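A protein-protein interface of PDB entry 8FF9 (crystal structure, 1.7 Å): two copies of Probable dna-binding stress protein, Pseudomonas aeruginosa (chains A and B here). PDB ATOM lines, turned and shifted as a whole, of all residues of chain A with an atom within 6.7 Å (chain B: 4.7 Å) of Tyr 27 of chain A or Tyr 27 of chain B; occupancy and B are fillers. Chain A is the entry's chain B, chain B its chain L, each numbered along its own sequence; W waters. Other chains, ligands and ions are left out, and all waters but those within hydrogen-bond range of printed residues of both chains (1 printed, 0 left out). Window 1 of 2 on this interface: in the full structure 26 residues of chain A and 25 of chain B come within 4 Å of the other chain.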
ATOM      1  N   LEU A  22     -10.536  28.748  -3.856  1.00  0.00           N
ATOM      2  CA  LEU A  22     -10.994  28.897  -5.240  1.00  0.00           C
ATOM      3  C   LEU A  22      -9.921  29.516  -6.126  1.00  0.00           C
ATOM      4  O   LEU A  22      -9.745  29.107  -7.282  1.00  0.00           O
ATOM      5  CB  LEU A  22     -12.252  29.761  -5.284  1.00  0.00           C
ATOM      6  CG  LEU A  22     -12.969  29.861  -6.621  1.00  0.00           C
ATOM      7  CD1 LEU A  22     -13.635  28.550  -6.931  1.00  0.00           C
ATOM      8  CD2 LEU A  22     -13.998  30.983  -6.621  1.00  0.00           C
ATOM      9  N   LEU A  23      -9.219  30.524  -5.617  1.00  0.00           N
ATOM     10  CA  LEU A  23      -8.116  31.136  -6.363  1.00  0.00           C
ATOM     11  C   LEU A  23      -7.036  30.115  -6.668  1.00  0.00           C
ATOM     12  O   LEU A  23      -6.522  30.050  -7.796  1.00  0.00           O
ATOM     13  CB  LEU A  23      -7.529  32.297  -5.556  1.00  0.00           C
ATOM     14  CG  LEU A  23      -6.330  33.041  -6.112  1.00  0.00           C
ATOM     15  CD1 LEU A  23      -6.677  33.601  -7.463  1.00  0.00           C
ATOM     16  CD2 LEU A  23      -5.884  34.144  -5.196  1.00  0.00           C
ATOM     17  N   ALA A  24      -6.643  29.324  -5.658  1.00  0.00           N
ATOM     18  CA  ALA A  24      -5.607  28.327  -5.876  1.00  0.00           C
ATOM     19  C   ALA A  24      -6.048  27.289  -6.903  1.00  0.00           C
ATOM     20  O   ALA A  24      -5.249  26.881  -7.750  1.00  0.00           O
ATOM     21  CB  ALA A  24      -5.230  27.639  -4.564  1.00  0.00           C
ATOM     22  N   ASP A  25      -7.294  26.827  -6.829  1.00  0.00           N
ATOM     23  CA  ASP A  25      -7.761  25.854  -7.818  1.00  0.00           C
ATOM     24  C   ASP A  25      -7.829  26.469  -9.219  1.00  0.00           C
ATOM     25  O   ASP A  25      -7.476  25.823 -10.221  1.00  0.00           O
ATOM     26  CB  ASP A  25      -9.113  25.285  -7.409  1.00  0.00           C
ATOM     27  CG  ASP A  25      -8.969  24.149  -6.404  1.00  0.00           C
ATOM     28  OD1 ASP A  25      -7.902  23.506  -6.420  1.00  0.00           O
ATOM     29  OD2 ASP A  25      -9.915  23.881  -5.637  1.00  0.00           O
ATOM     30  N   THR A  26      -8.304  27.704  -9.307  1.00  0.00           N
ATOM     31  CA  THR A  26      -8.355  28.366 -10.599  1.00  0.00           C
ATOM     32  C   THR A  26      -6.952  28.519 -11.164  1.00  0.00           C
ATOM     33  O   THR A  26      -6.732  28.278 -12.353  1.00  0.00           O
ATOM     34  CB  THR A  26      -9.044  29.724 -10.466  1.00  0.00           C
ATOM     35  OG1 THR A  26     -10.365  29.533  -9.963  1.00  0.00           O
ATOM     36  CG2 THR A  26      -9.149  30.419 -11.831  1.00  0.00           C
ATOM     37  N   TYR A  27      -5.990  28.912 -10.320  1.00  0.00           N
ATOM     38  CA  TYR A  27      -4.619  29.080 -10.785  1.00  0.00           C
ATOM     39  C   TYR A  27      -4.003  27.737 -11.178  1.00  0.00           C
ATOM     40  O   TYR A  27      -3.260  27.656 -12.161  1.00  0.00           O
ATOM     41  CB  TYR A  27      -3.769  29.781  -9.712  1.00  0.00           C
ATOM     42  CG  TYR A  27      -2.566  30.410 -10.338  1.00  0.00           C
ATOM     43  CD1 TYR A  27      -1.440  29.658 -10.610  1.00  0.00           C
ATOM     44  CD2 TYR A  27      -2.600  31.726 -10.754  1.00  0.00           C
ATOM     45  CE1 TYR A  27      -0.360  30.207 -11.246  1.00  0.00           C
ATOM     46  CE2 TYR A  27      -1.507  32.289 -11.396  1.00  0.00           C
ATOM     47  CZ  TYR A  27      -0.410  31.533 -11.634  1.00  0.00           C
ATOM     48  OH  TYR A  27       0.692  32.074 -12.267  1.00  0.00           O
ATOM     49  N   THR A  28      -4.304  26.667 -10.430  1.00  0.00           N
ATOM     50  CA  THR A  28      -3.762  25.355 -10.781  1.00  0.00           C
ATOM     51  C   THR A  28      -4.311  24.895 -12.125  1.00  0.00           C
ATOM     52  O   THR A  28      -3.560  24.396 -12.978  1.00  0.00           O
ATOM     53  CB  THR A  28      -4.070  24.341  -9.680  1.00  0.00           C
ATOM     54  OG1 THR A  28      -3.585  24.840  -8.419  1.00  0.00           O
ATOM     55  CG2 THR A  28      -3.377  22.996  -9.964  1.00  0.00           C
ATOM     56  N   LEU A  29      -5.610  25.081 -12.343  1.00  0.00           N
ATOM     57  CA  LEU A  29      -6.192  24.739 -13.636  1.00  0.00           C
ATOM     58  C   LEU A  29      -5.634  25.627 -14.742  1.00  0.00           C
ATOM     59  O   LEU A  29      -5.420  25.166 -15.872  1.00  0.00           O
ATOM     60  CB  LEU A  29      -7.713  24.856 -13.570  1.00  0.00           C
ATOM     61  CG  LEU A  29      -8.465  24.432 -14.821  1.00  0.00           C
ATOM     62  CD1 LEU A  29      -8.182  22.984 -15.158  1.00  0.00           C
ATOM     63  CD2 LEU A  29      -9.962  24.675 -14.626  1.00  0.00           C
ATOM     64  N   TYR A  30      -5.421  26.909 -14.445  1.00  0.00           N
ATOM     65  CA  TYR A  30      -4.769  27.812 -15.388  1.00  0.00           C
ATOM     66  C   TYR A  30      -3.427  27.262 -15.840  1.00  0.00           C
ATOM     67  O   TYR A  30      -3.155  27.154 -17.045  1.00  0.00           O
ATOM     68  CB  TYR A  30      -4.629  29.185 -14.730  1.00  0.00           C
ATOM     69  CG  TYR A  30      -3.739  30.191 -15.396  1.00  0.00           C
ATOM     70  CD1 TYR A  30      -3.938  30.577 -16.703  1.00  0.00           C
ATOM     71  CD2 TYR A  30      -2.746  30.818 -14.676  1.00  0.00           C
ATOM     72  CE1 TYR A  30      -3.120  31.530 -17.303  1.00  0.00           C
ATOM     73  CE2 TYR A  30      -1.943  31.781 -15.252  1.00  0.00           C
ATOM     74  CZ  TYR A  30      -2.128  32.123 -16.573  1.00  0.00           C
ATOM     75  OH  TYR A  30      -1.327  33.080 -17.165  1.00  0.00           O
ATOM     76  N   LEU A  31      -2.566  26.899 -14.895  1.00  0.00           N
ATOM     77  CA  LEU A  31      -1.242  26.425 -15.269  1.00  0.00           C
ATOM     78  C   LEU A  31      -1.315  25.079 -15.988  1.00  0.00           C
ATOM     79  O   LEU A  31      -0.564  24.840 -16.947  1.00  0.00           O
ATOM     80  CB  LEU A  31      -0.362  26.336 -14.021  1.00  0.00           C
ATOM     81  CG  LEU A  31       1.061  25.851 -14.255  1.00  0.00           C
ATOM     82  CD1 LEU A  31       1.807  26.714 -15.268  1.00  0.00           C
ATOM     83  CD2 LEU A  31       1.813  25.821 -12.919  1.00  0.00           C
ATOM     84  N   LYS A  32      -2.196  24.180 -15.540  1.00  0.00           N
ATOM     85  CA  LYS A  32      -2.346  22.902 -16.234  1.00  0.00           C
ATOM     86  C   LYS A  32      -2.811  23.115 -17.676  1.00  0.00           C
ATOM     87  O   LYS A  32      -2.312  22.465 -18.603  1.00  0.00           O
ATOM     88  CB  LYS A  32      -3.325  21.978 -15.491  1.00  0.00           C
ATOM     89  CG  LYS A  32      -3.495  20.635 -16.211  1.00  0.00           C
ATOM     90  CD  LYS A  32      -4.489  19.661 -15.548  1.00  0.00           C
ATOM     91  CE  LYS A  32      -3.967  19.066 -14.289  1.00  0.00           C
ATOM     92  NZ  LYS A  32      -4.730  17.811 -13.882  1.00  0.00           N
ATOM     93  N   HIS A  34      -2.408  25.788 -19.513  1.00  0.00           N
ATOM     94  CA  HIS A  34      -1.303  26.404 -20.241  1.00  0.00           C
ATOM     95  C   HIS A  34      -0.256  25.365 -20.626  1.00  0.00           C
ATOM     96  O   HIS A  34       0.239  25.345 -21.762  1.00  0.00           O
ATOM     97  CB  HIS A  34      -0.686  27.487 -19.350  1.00  0.00           C
ATOM     98  CG  HIS A  34      -0.069  28.618 -20.093  1.00  0.00           C
ATOM     99  ND1 HIS A  34       0.274  29.801 -19.476  1.00  0.00           N
ATOM    100  CD2 HIS A  34       0.277  28.749 -21.393  1.00  0.00           C
ATOM    101  CE1 HIS A  34       0.793  30.619 -20.373  1.00  0.00           C
ATOM    102  NE2 HIS A  34       0.813  30.005 -21.538  1.00  0.00           N
ATOM    103  N   TRP A  38       0.986  24.107 -24.518  1.00  0.00           N
ATOM    104  CA  TRP A  38       2.315  23.941 -25.071  1.00  0.00           C
ATOM    105  C   TRP A  38       2.573  22.520 -25.552  1.00  0.00           C
ATOM    106  O   TRP A  38       3.275  22.325 -26.557  1.00  0.00           O
ATOM    107  CB  TRP A  38       3.373  24.294 -24.039  1.00  0.00           C
ATOM    108  CG  TRP A  38       3.331  25.681 -23.512  1.00  0.00           C
ATOM    109  CD1 TRP A  38       3.043  26.821 -24.188  1.00  0.00           C
ATOM    110  CD2 TRP A  38       3.604  26.069 -22.161  1.00  0.00           C
ATOM    111  NE1 TRP A  38       3.123  27.911 -23.343  1.00  0.00           N
ATOM    112  CE2 TRP A  38       3.463  27.469 -22.090  1.00  0.00           C
ATOM    113  CE3 TRP A  38       3.973  25.359 -21.006  1.00  0.00           C
ATOM    114  CZ2 TRP A  38       3.677  28.179 -20.916  1.00  0.00           C
ATOM    115  CZ3 TRP A  38       4.177  26.070 -19.827  1.00  0.00           C
ATOM    116  CH2 TRP A  38       4.020  27.461 -19.795  1.00  0.00           C
ATOM    117  N   LEU A  59      -8.921  32.021 -17.890  1.00  0.00           N
ATOM    118  CA  LEU A  59      -8.613  31.732 -16.488  1.00  0.00           C
ATOM    119  C   LEU A  59      -7.685  32.768 -15.883  1.00  0.00           C
ATOM    120  O   LEU A  59      -7.804  33.076 -14.694  1.00  0.00           O
ATOM    121  CB  LEU A  59      -8.005  30.339 -16.346  1.00  0.00           C
ATOM    122  CG  LEU A  59      -8.962  29.199 -16.676  1.00  0.00           C
ATOM    123  CD1 LEU A  59      -8.260  27.878 -16.751  1.00  0.00           C
ATOM    124  CD2 LEU A  59     -10.129  29.085 -15.680  1.00  0.00           C
ATOM    125  N   VAL A  63      -8.447  34.565 -12.323  1.00  0.00           N
ATOM    126  CA  VAL A  63      -7.609  34.626 -11.139  1.00  0.00           C
ATOM    127  C   VAL A  63      -7.512  36.053 -10.618  1.00  0.00           C
ATOM    128  O   VAL A  63      -7.582  36.281  -9.409  1.00  0.00           O
ATOM    129  CB  VAL A  63      -6.212  34.018 -11.368  1.00  0.00           C
ATOM    130  CG1 VAL A  63      -6.319  32.522 -11.682  1.00  0.00           C
ATOM    131  CG2 VAL A  63      -5.439  34.756 -12.424  1.00  0.00           C
ATOM    132  N   ILE A  66     -10.898  36.877  -8.849  1.00  0.00           N
ATOM    133  CA  ILE A  66     -11.023  36.249  -7.538  1.00  0.00           C
ATOM    134  C   ILE A  66     -10.116  36.933  -6.531  1.00  0.00           C
ATOM    135  O   ILE A  66     -10.535  37.257  -5.412  1.00  0.00           O
ATOM    136  CB  ILE A  66     -10.724  34.737  -7.634  1.00  0.00           C
ATOM    137  CG1 ILE A  66     -11.756  34.059  -8.520  1.00  0.00           C
ATOM    138  CG2 ILE A  66     -10.771  34.119  -6.244  1.00  0.00           C
ATOM    139  CD1 ILE A  66     -11.322  32.692  -9.042  1.00  0.00           C
ATOM    140  N   TYR A  81       3.679  29.484  -5.178  1.00  0.00           N
ATOM    141  CA  TYR A  81       3.558  28.039  -5.354  1.00  0.00           C
ATOM    142  C   TYR A  81       3.213  27.342  -4.047  1.00  0.00           C
ATOM    143  O   TYR A  81       2.378  26.431  -4.020  1.00  0.00           O
ATOM    144  CB  TYR A  81       4.851  27.444  -5.898  1.00  0.00           C
ATOM    145  CG  TYR A  81       5.299  28.013  -7.228  1.00  0.00           C
ATOM    146  CD1 TYR A  81       4.382  28.403  -8.182  1.00  0.00           C
ATOM    147  CD2 TYR A  81       6.652  28.157  -7.515  1.00  0.00           C
ATOM    148  CE1 TYR A  81       4.804  28.936  -9.397  1.00  0.00           C
ATOM    149  CE2 TYR A  81       7.077  28.692  -8.733  1.00  0.00           C
ATOM    150  CZ  TYR A  81       6.131  29.063  -9.659  1.00  0.00           C
ATOM    151  OH  TYR A  81       6.527  29.607 -10.852  1.00  0.00           O
ATOM    152  N   TYR A  84      -0.399  27.976  -3.151  1.00  0.00           N
ATOM    153  CA  TYR A  84      -1.355  27.321  -4.038  1.00  0.00           C
ATOM    154  C   TYR A  84      -1.275  25.805  -3.946  1.00  0.00           C
ATOM    155  O   TYR A  84      -2.295  25.123  -4.079  1.00  0.00           O
ATOM    156  CB  TYR A  84      -1.133  27.777  -5.477  1.00  0.00           C
ATOM    157  CG  TYR A  84      -1.528  29.213  -5.765  1.00  0.00           C
ATOM    158  CD1 TYR A  84      -2.275  29.959  -4.864  1.00  0.00           C
ATOM    159  CD2 TYR A  84      -1.150  29.822  -6.952  1.00  0.00           C
ATOM    160  CE1 TYR A  84      -2.630  31.270  -5.152  1.00  0.00           C
ATOM    161  CE2 TYR A  84      -1.495  31.130  -7.234  1.00  0.00           C
ATOM    162  CZ  TYR A  84      -2.238  31.847  -6.340  1.00  0.00           C
ATOM    163  OH  TYR A  84      -2.571  33.146  -6.655  1.00  0.00           O
ATOM    164  N   GLU A  92      -1.772  18.110 -10.176  1.00  0.00           N
ATOM    165  CA  GLU A  92      -1.092  18.505 -11.393  1.00  0.00           C
ATOM    166  C   GLU A  92      -0.547  17.283 -12.122  1.00  0.00           C
ATOM    167  O   GLU A  92      -0.241  16.240 -11.527  1.00  0.00           O
ATOM    168  CB  GLU A  92       0.031  19.479 -11.076  1.00  0.00           C
ATOM    169  CG  GLU A  92      -0.455  20.845 -10.622  1.00  0.00           C
ATOM    170  CD  GLU A  92       0.695  21.753 -10.338  1.00  0.00           C
ATOM    171  OE1 GLU A  92       1.354  21.584  -9.279  1.00  0.00           O
ATOM    172  OE2 GLU A  92       0.964  22.593 -11.196  1.00  0.00           O
ATOM    173  N   LEU B  23      12.358  29.544 -18.147  1.00  0.00           N
ATOM    174  CA  LEU B  23      10.898  29.515 -18.074  1.00  0.00           C
ATOM    175  C   LEU B  23      10.426  29.538 -16.625  1.00  0.00           C
ATOM    176  O   LEU B  23       9.538  30.323 -16.252  1.00  0.00           O
ATOM    177  CB  LEU B  23      10.373  28.276 -18.809  1.00  0.00           C
ATOM    178  CG  LEU B  23       8.872  28.019 -18.764  1.00  0.00           C
ATOM    179  CD1 LEU B  23       8.138  29.193 -19.336  1.00  0.00           C
ATOM    180  CD2 LEU B  23       8.495  26.744 -19.549  1.00  0.00           C
ATOM    181  N   ALA B  24      11.031  28.711 -15.787  1.00  0.00           N
ATOM    182  CA  ALA B  24      10.638  28.671 -14.380  1.00  0.00           C
ATOM    183  C   ALA B  24      10.884  30.014 -13.692  1.00  0.00           C
ATOM    184  O   ALA B  24      10.035  30.492 -12.928  1.00  0.00           O
ATOM    185  CB  ALA B  24      11.379  27.552 -13.658  1.00  0.00           C
ATOM    186  N   ASP B  25      12.038  30.634 -13.937  1.00  0.00           N
ATOM    187  CA  ASP B  25      12.306  31.936 -13.338  1.00  0.00           C
ATOM    188  C   ASP B  25      11.314  32.979 -13.834  1.00  0.00           C
ATOM    189  O   ASP B  25      10.801  33.792 -13.049  1.00  0.00           O
ATOM    190  CB  ASP B  25      13.732  32.378 -13.649  1.00  0.00           C
ATOM    191  CG  ASP B  25      14.758  31.630 -12.821  1.00  0.00           C
ATOM    192  OD1 ASP B  25      14.406  31.146 -11.744  1.00  0.00           O
ATOM    193  OD2 ASP B  25      15.913  31.517 -13.243  1.00  0.00           O
ATOM    194  N   THR B  26      11.052  32.989 -15.144  1.00  0.00           N
ATOM    195  CA  THR B  26      10.109  33.955 -15.693  1.00  0.00           C
ATOM    196  C   THR B  26       8.718  33.724 -15.140  1.00  0.00           C
ATOM    197  O   THR B  26       8.015  34.676 -14.781  1.00  0.00           O
ATOM    198  CB  THR B  26      10.088  33.859 -17.217  1.00  0.00           C
ATOM    199  OG1 THR B  26      11.417  34.041 -17.705  1.00  0.00           O
ATOM    200  CG2 THR B  26       9.162  34.900 -17.829  1.00  0.00           C
ATOM    201  N   TYR B  27       8.308  32.464 -15.039  1.00  0.00           N
ATOM    202  CA  TYR B  27       6.969  32.192 -14.540  1.00  0.00           C
ATOM    203  C   TYR B  27       6.863  32.542 -13.057  1.00  0.00           C
ATOM    204  O   TYR B  27       5.822  33.042 -12.593  1.00  0.00           O
ATOM    205  CB  TYR B  27       6.606  30.733 -14.788  1.00  0.00           C
ATOM    206  CG  TYR B  27       5.150  30.571 -14.672  1.00  0.00           C
ATOM    207  CD1 TYR B  27       4.547  30.520 -13.413  1.00  0.00           C
ATOM    208  CD2 TYR B  27       4.364  30.579 -15.787  1.00  0.00           C
ATOM    209  CE1 TYR B  27       3.176  30.424 -13.283  1.00  0.00           C
ATOM    210  CE2 TYR B  27       2.981  30.485 -15.688  1.00  0.00           C
ATOM    211  CZ  TYR B  27       2.391  30.407 -14.444  1.00  0.00           C
ATOM    212  OH  TYR B  27       1.012  30.329 -14.365  1.00  0.00           O
ATOM    213  N   THR B  28       7.915  32.273 -12.297  1.00  0.00           N
ATOM    214  CA  THR B  28       7.891  32.587 -10.873  1.00  0.00           C
ATOM    215  C   THR B  28       7.859  34.096 -10.656  1.00  0.00           C
ATOM    216  O   THR B  28       7.136  34.587  -9.787  1.00  0.00           O
ATOM    217  CB  THR B  28       9.092  31.945 -10.191  1.00  0.00           C
ATOM    218  OG1 THR B  28       9.063  30.528 -10.439  1.00  0.00           O
ATOM    219  CG2 THR B  28       9.070  32.186  -8.687  1.00  0.00           C
ATOM    220  N   LEU B  29       8.605  34.846 -11.464  1.00  0.00           N
ATOM    221  CA  LEU B  29       8.530  36.307 -11.423  1.00  0.00           C
ATOM    222  C   LEU B  29       7.161  36.798 -11.851  1.00  0.00           C
ATOM    223  O   LEU B  29       6.651  37.781 -11.306  1.00  0.00           O
ATOM    224  CB  LEU B  29       9.624  36.897 -12.305  1.00  0.00           C
ATOM    225  CG  LEU B  29       9.730  38.418 -12.308  1.00  0.00           C
ATOM    226  CD1 LEU B  29       9.941  38.928 -10.881  1.00  0.00           C
ATOM    227  CD2 LEU B  29      10.879  38.813 -13.212  1.00  0.00           C
ATOM    228  N   TYR B  30       6.554  36.140 -12.850  1.00  0.00           N
ATOM    229  CA  TYR B  30       5.199  36.480 -13.269  1.00  0.00           C
ATOM    230  C   TYR B  30       4.239  36.402 -12.098  1.00  0.00           C
ATOM    231  O   TYR B  30       3.505  37.363 -11.810  1.00  0.00           O
ATOM    232  CB  TYR B  30       4.788  35.531 -14.401  1.00  0.00           C
ATOM    233  CG  TYR B  30       3.337  35.480 -14.797  1.00  0.00           C
ATOM    234  CD1 TYR B  30       2.659  36.603 -15.187  1.00  0.00           C
ATOM    235  CD2 TYR B  30       2.676  34.272 -14.857  1.00  0.00           C
ATOM    236  CE1 TYR B  30       1.338  36.548 -15.585  1.00  0.00           C
ATOM    237  CE2 TYR B  30       1.344  34.197 -15.254  1.00  0.00           C
ATOM    238  CZ  TYR B  30       0.683  35.348 -15.613  1.00  0.00           C
ATOM    239  OH  TYR B  30      -0.638  35.319 -16.000  1.00  0.00           O
ATOM    240  N   LEU B  31       4.253  35.276 -11.385  1.00  0.00           N
ATOM    241  CA  LEU B  31       3.314  35.139 -10.277  1.00  0.00           C
ATOM    242  C   LEU B  31       3.653  36.108  -9.151  1.00  0.00           C
ATOM    243  O   LEU B  31       2.744  36.683  -8.534  1.00  0.00           O
ATOM    244  CB  LEU B  31       3.296  33.702  -9.770  1.00  0.00           C
ATOM    245  CG  LEU B  31       2.424  33.438  -8.544  1.00  0.00           C
ATOM    246  CD1 LEU B  31       0.969  33.826  -8.784  1.00  0.00           C
ATOM    247  CD2 LEU B  31       2.527  31.962  -8.187  1.00  0.00           C
ATOM    248  N   VAL B  63       6.480  33.897 -21.128  1.00  0.00           N
ATOM    249  CA  VAL B  63       6.490  32.466 -20.816  1.00  0.00           C
ATOM    250  C   VAL B  63       6.083  31.649 -22.035  1.00  0.00           C
ATOM    251  O   VAL B  63       6.623  30.564 -22.271  1.00  0.00           O
ATOM    252  CB  VAL B  63       5.611  32.133 -19.594  1.00  0.00           C
ATOM    253  CG1 VAL B  63       6.120  32.853 -18.345  1.00  0.00           C
ATOM    254  CG2 VAL B  63       4.140  32.412 -19.838  1.00  0.00           C
ATOM    255  N   TYR B  81       3.792  23.395 -10.341  1.00  0.00           N
ATOM    256  CA  TYR B  81       4.420  23.999  -9.165  1.00  0.00           C
ATOM    257  C   TYR B  81       5.705  23.277  -8.785  1.00  0.00           C
ATOM    258  O   TYR B  81       6.688  23.917  -8.398  1.00  0.00           O
ATOM    259  CB  TYR B  81       3.472  23.970  -7.971  1.00  0.00           C
ATOM    260  CG  TYR B  81       2.173  24.697  -8.176  1.00  0.00           C
ATOM    261  CD1 TYR B  81       2.086  25.807  -9.016  1.00  0.00           C
ATOM    262  CD2 TYR B  81       1.021  24.244  -7.558  1.00  0.00           C
ATOM    263  CE1 TYR B  81       0.856  26.474  -9.201  1.00  0.00           C
ATOM    264  CE2 TYR B  81      -0.192  24.888  -7.732  1.00  0.00           C
ATOM    265  CZ  TYR B  81      -0.266  25.995  -8.561  1.00  0.00           C
ATOM    266  OH  TYR B  81      -1.462  26.638  -8.734  1.00  0.00           O
ATOM    267  N   TYR B  84       8.547  24.049 -11.354  1.00  0.00           N
ATOM    268  CA  TYR B  84       9.064  25.408 -11.277  1.00  0.00           C
ATOM    269  C   TYR B  84       9.755  25.680  -9.942  1.00  0.00           C
ATOM    270  O   TYR B  84      10.722  26.443  -9.896  1.00  0.00           O
ATOM    271  CB  TYR B  84       7.948  26.422 -11.531  1.00  0.00           C
ATOM    272  CG  TYR B  84       7.410  26.468 -12.948  1.00  0.00           C
ATOM    273  CD1 TYR B  84       8.076  25.860 -14.003  1.00  0.00           C
ATOM    274  CD2 TYR B  84       6.244  27.159 -13.229  1.00  0.00           C
ATOM    275  CE1 TYR B  84       7.564  25.926 -15.302  1.00  0.00           C
ATOM    276  CE2 TYR B  84       5.729  27.227 -14.518  1.00  0.00           C
ATOM    277  CZ  TYR B  84       6.398  26.614 -15.541  1.00  0.00           C
ATOM    278  OH  TYR B  84       5.883  26.689 -16.825  1.00  0.00           O
HETATM  279  O   HOH W   1      -0.385  29.487 -16.478  1.00  0.00           O
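N of Tyr 81 of chain B lies within hydrogen-bond range of OE2 of Glu 92 of chain A (3.1 Å).
The side-chain hydroxyl (OH) of Tyr 30 of chain B lies within hydrogen-bond range of the side-chain hydroxyl (OH) of Tyr 30 of chain A (2.6 Å).
The side-chain hydroxyl of Thr 28 of chain A is in hydrogen-bond range of the side-chain hydroxyl of Tyr 81 of chain B (2.8 Å).
OH of Tyr 81 of chain A lies within hydrogen-bond range of OG1 of Thr 28 of chain B.
OH of Tyr 27 of chain A sits at hydrogen-bond distance from OH of Tyr 27 of chain B (2.7 Å).
The backbone carbonyl oxygen (O) of Ala 24 of chain A sits at hydrogen-bond distance from the side-chain hydroxyl (OG1) of Thr 28 of chain A (2.7 Å).
The side-chain hydroxyl (OG1) of Thr 28 of chain B lies within hydrogen-bond range of the backbone carbonyl oxygen (O) of Ala 24 of chain B.
Tyr 30 of chain B touches Tyr 27 of chain A.
Tyr 27 of chain A touches Leu 31 of chain B.
CD1 of Leu 31 of chain A touches OH of Tyr 27 of chain B (3.8 Å).
CE1 of Tyr 81 of chain B touches CD2 of Leu 31 of chain A (3.9 Å).
His 34 of chain A touches Val 63 of chain B (CE1 to CG2, 3.8 Å).
Tyr 27 of chain B touches Tyr 81 of chain A.
Tyr 81 of chain A touches Tyr 81 of chain B.
Tyr 81 of chain A touches Tyr 84 of chain B (OH to CD2, 3.4 Å).
Tyr 84 of chain A touches Leu 31 of chain B.
CB of Tyr 84 of chain A touches OH of Tyr 81 of chain B, 3.5 Å away.
Of the printed residues of chain B, Thr 28 of chain A touches Tyr 81 (2.8 Å).
Of the printed residues of chain B, Tyr 84 of chain A touches Leu 31 and Tyr 81.
Of the 19 printed residues of chain A, 10 touch a printed residue of chain B.
Printed residues of chain A that touch a printed residue of chain B: Ala 24, Tyr 27, Thr 28, Tyr 30, Leu 31, His 34, Trp 38, Tyr 81, Tyr 84 and Glu 92.
Among the printed residues, no Asp or Glu carboxylate lies within 4 Å of a Lys or Arg side-chain nitrogen of the other chain.
Tyr 27 of chain A touches its own counterpart, Tyr 27 of chain B.
Tyr 27 of chain A touches Leu 31 of chain B, and with the chains exchanged Leu 31 of chain A touches Tyr 27 of chain B.
Thr 28 of chain A touches Tyr 81 of chain B, and with the chains exchanged Tyr 81 of chain A touches Thr 28 of chain B.
Tyr 84 of chain A touches Leu 31 of chain B, but with the chains exchanged Leu 31 of chain A does not touch Tyr 84 of chain B (4.03 Å).
12 positions are printed for both chains.
Water W1 bridges OH of Tyr 27 of chain B and ND1 of His 34 of chain A.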
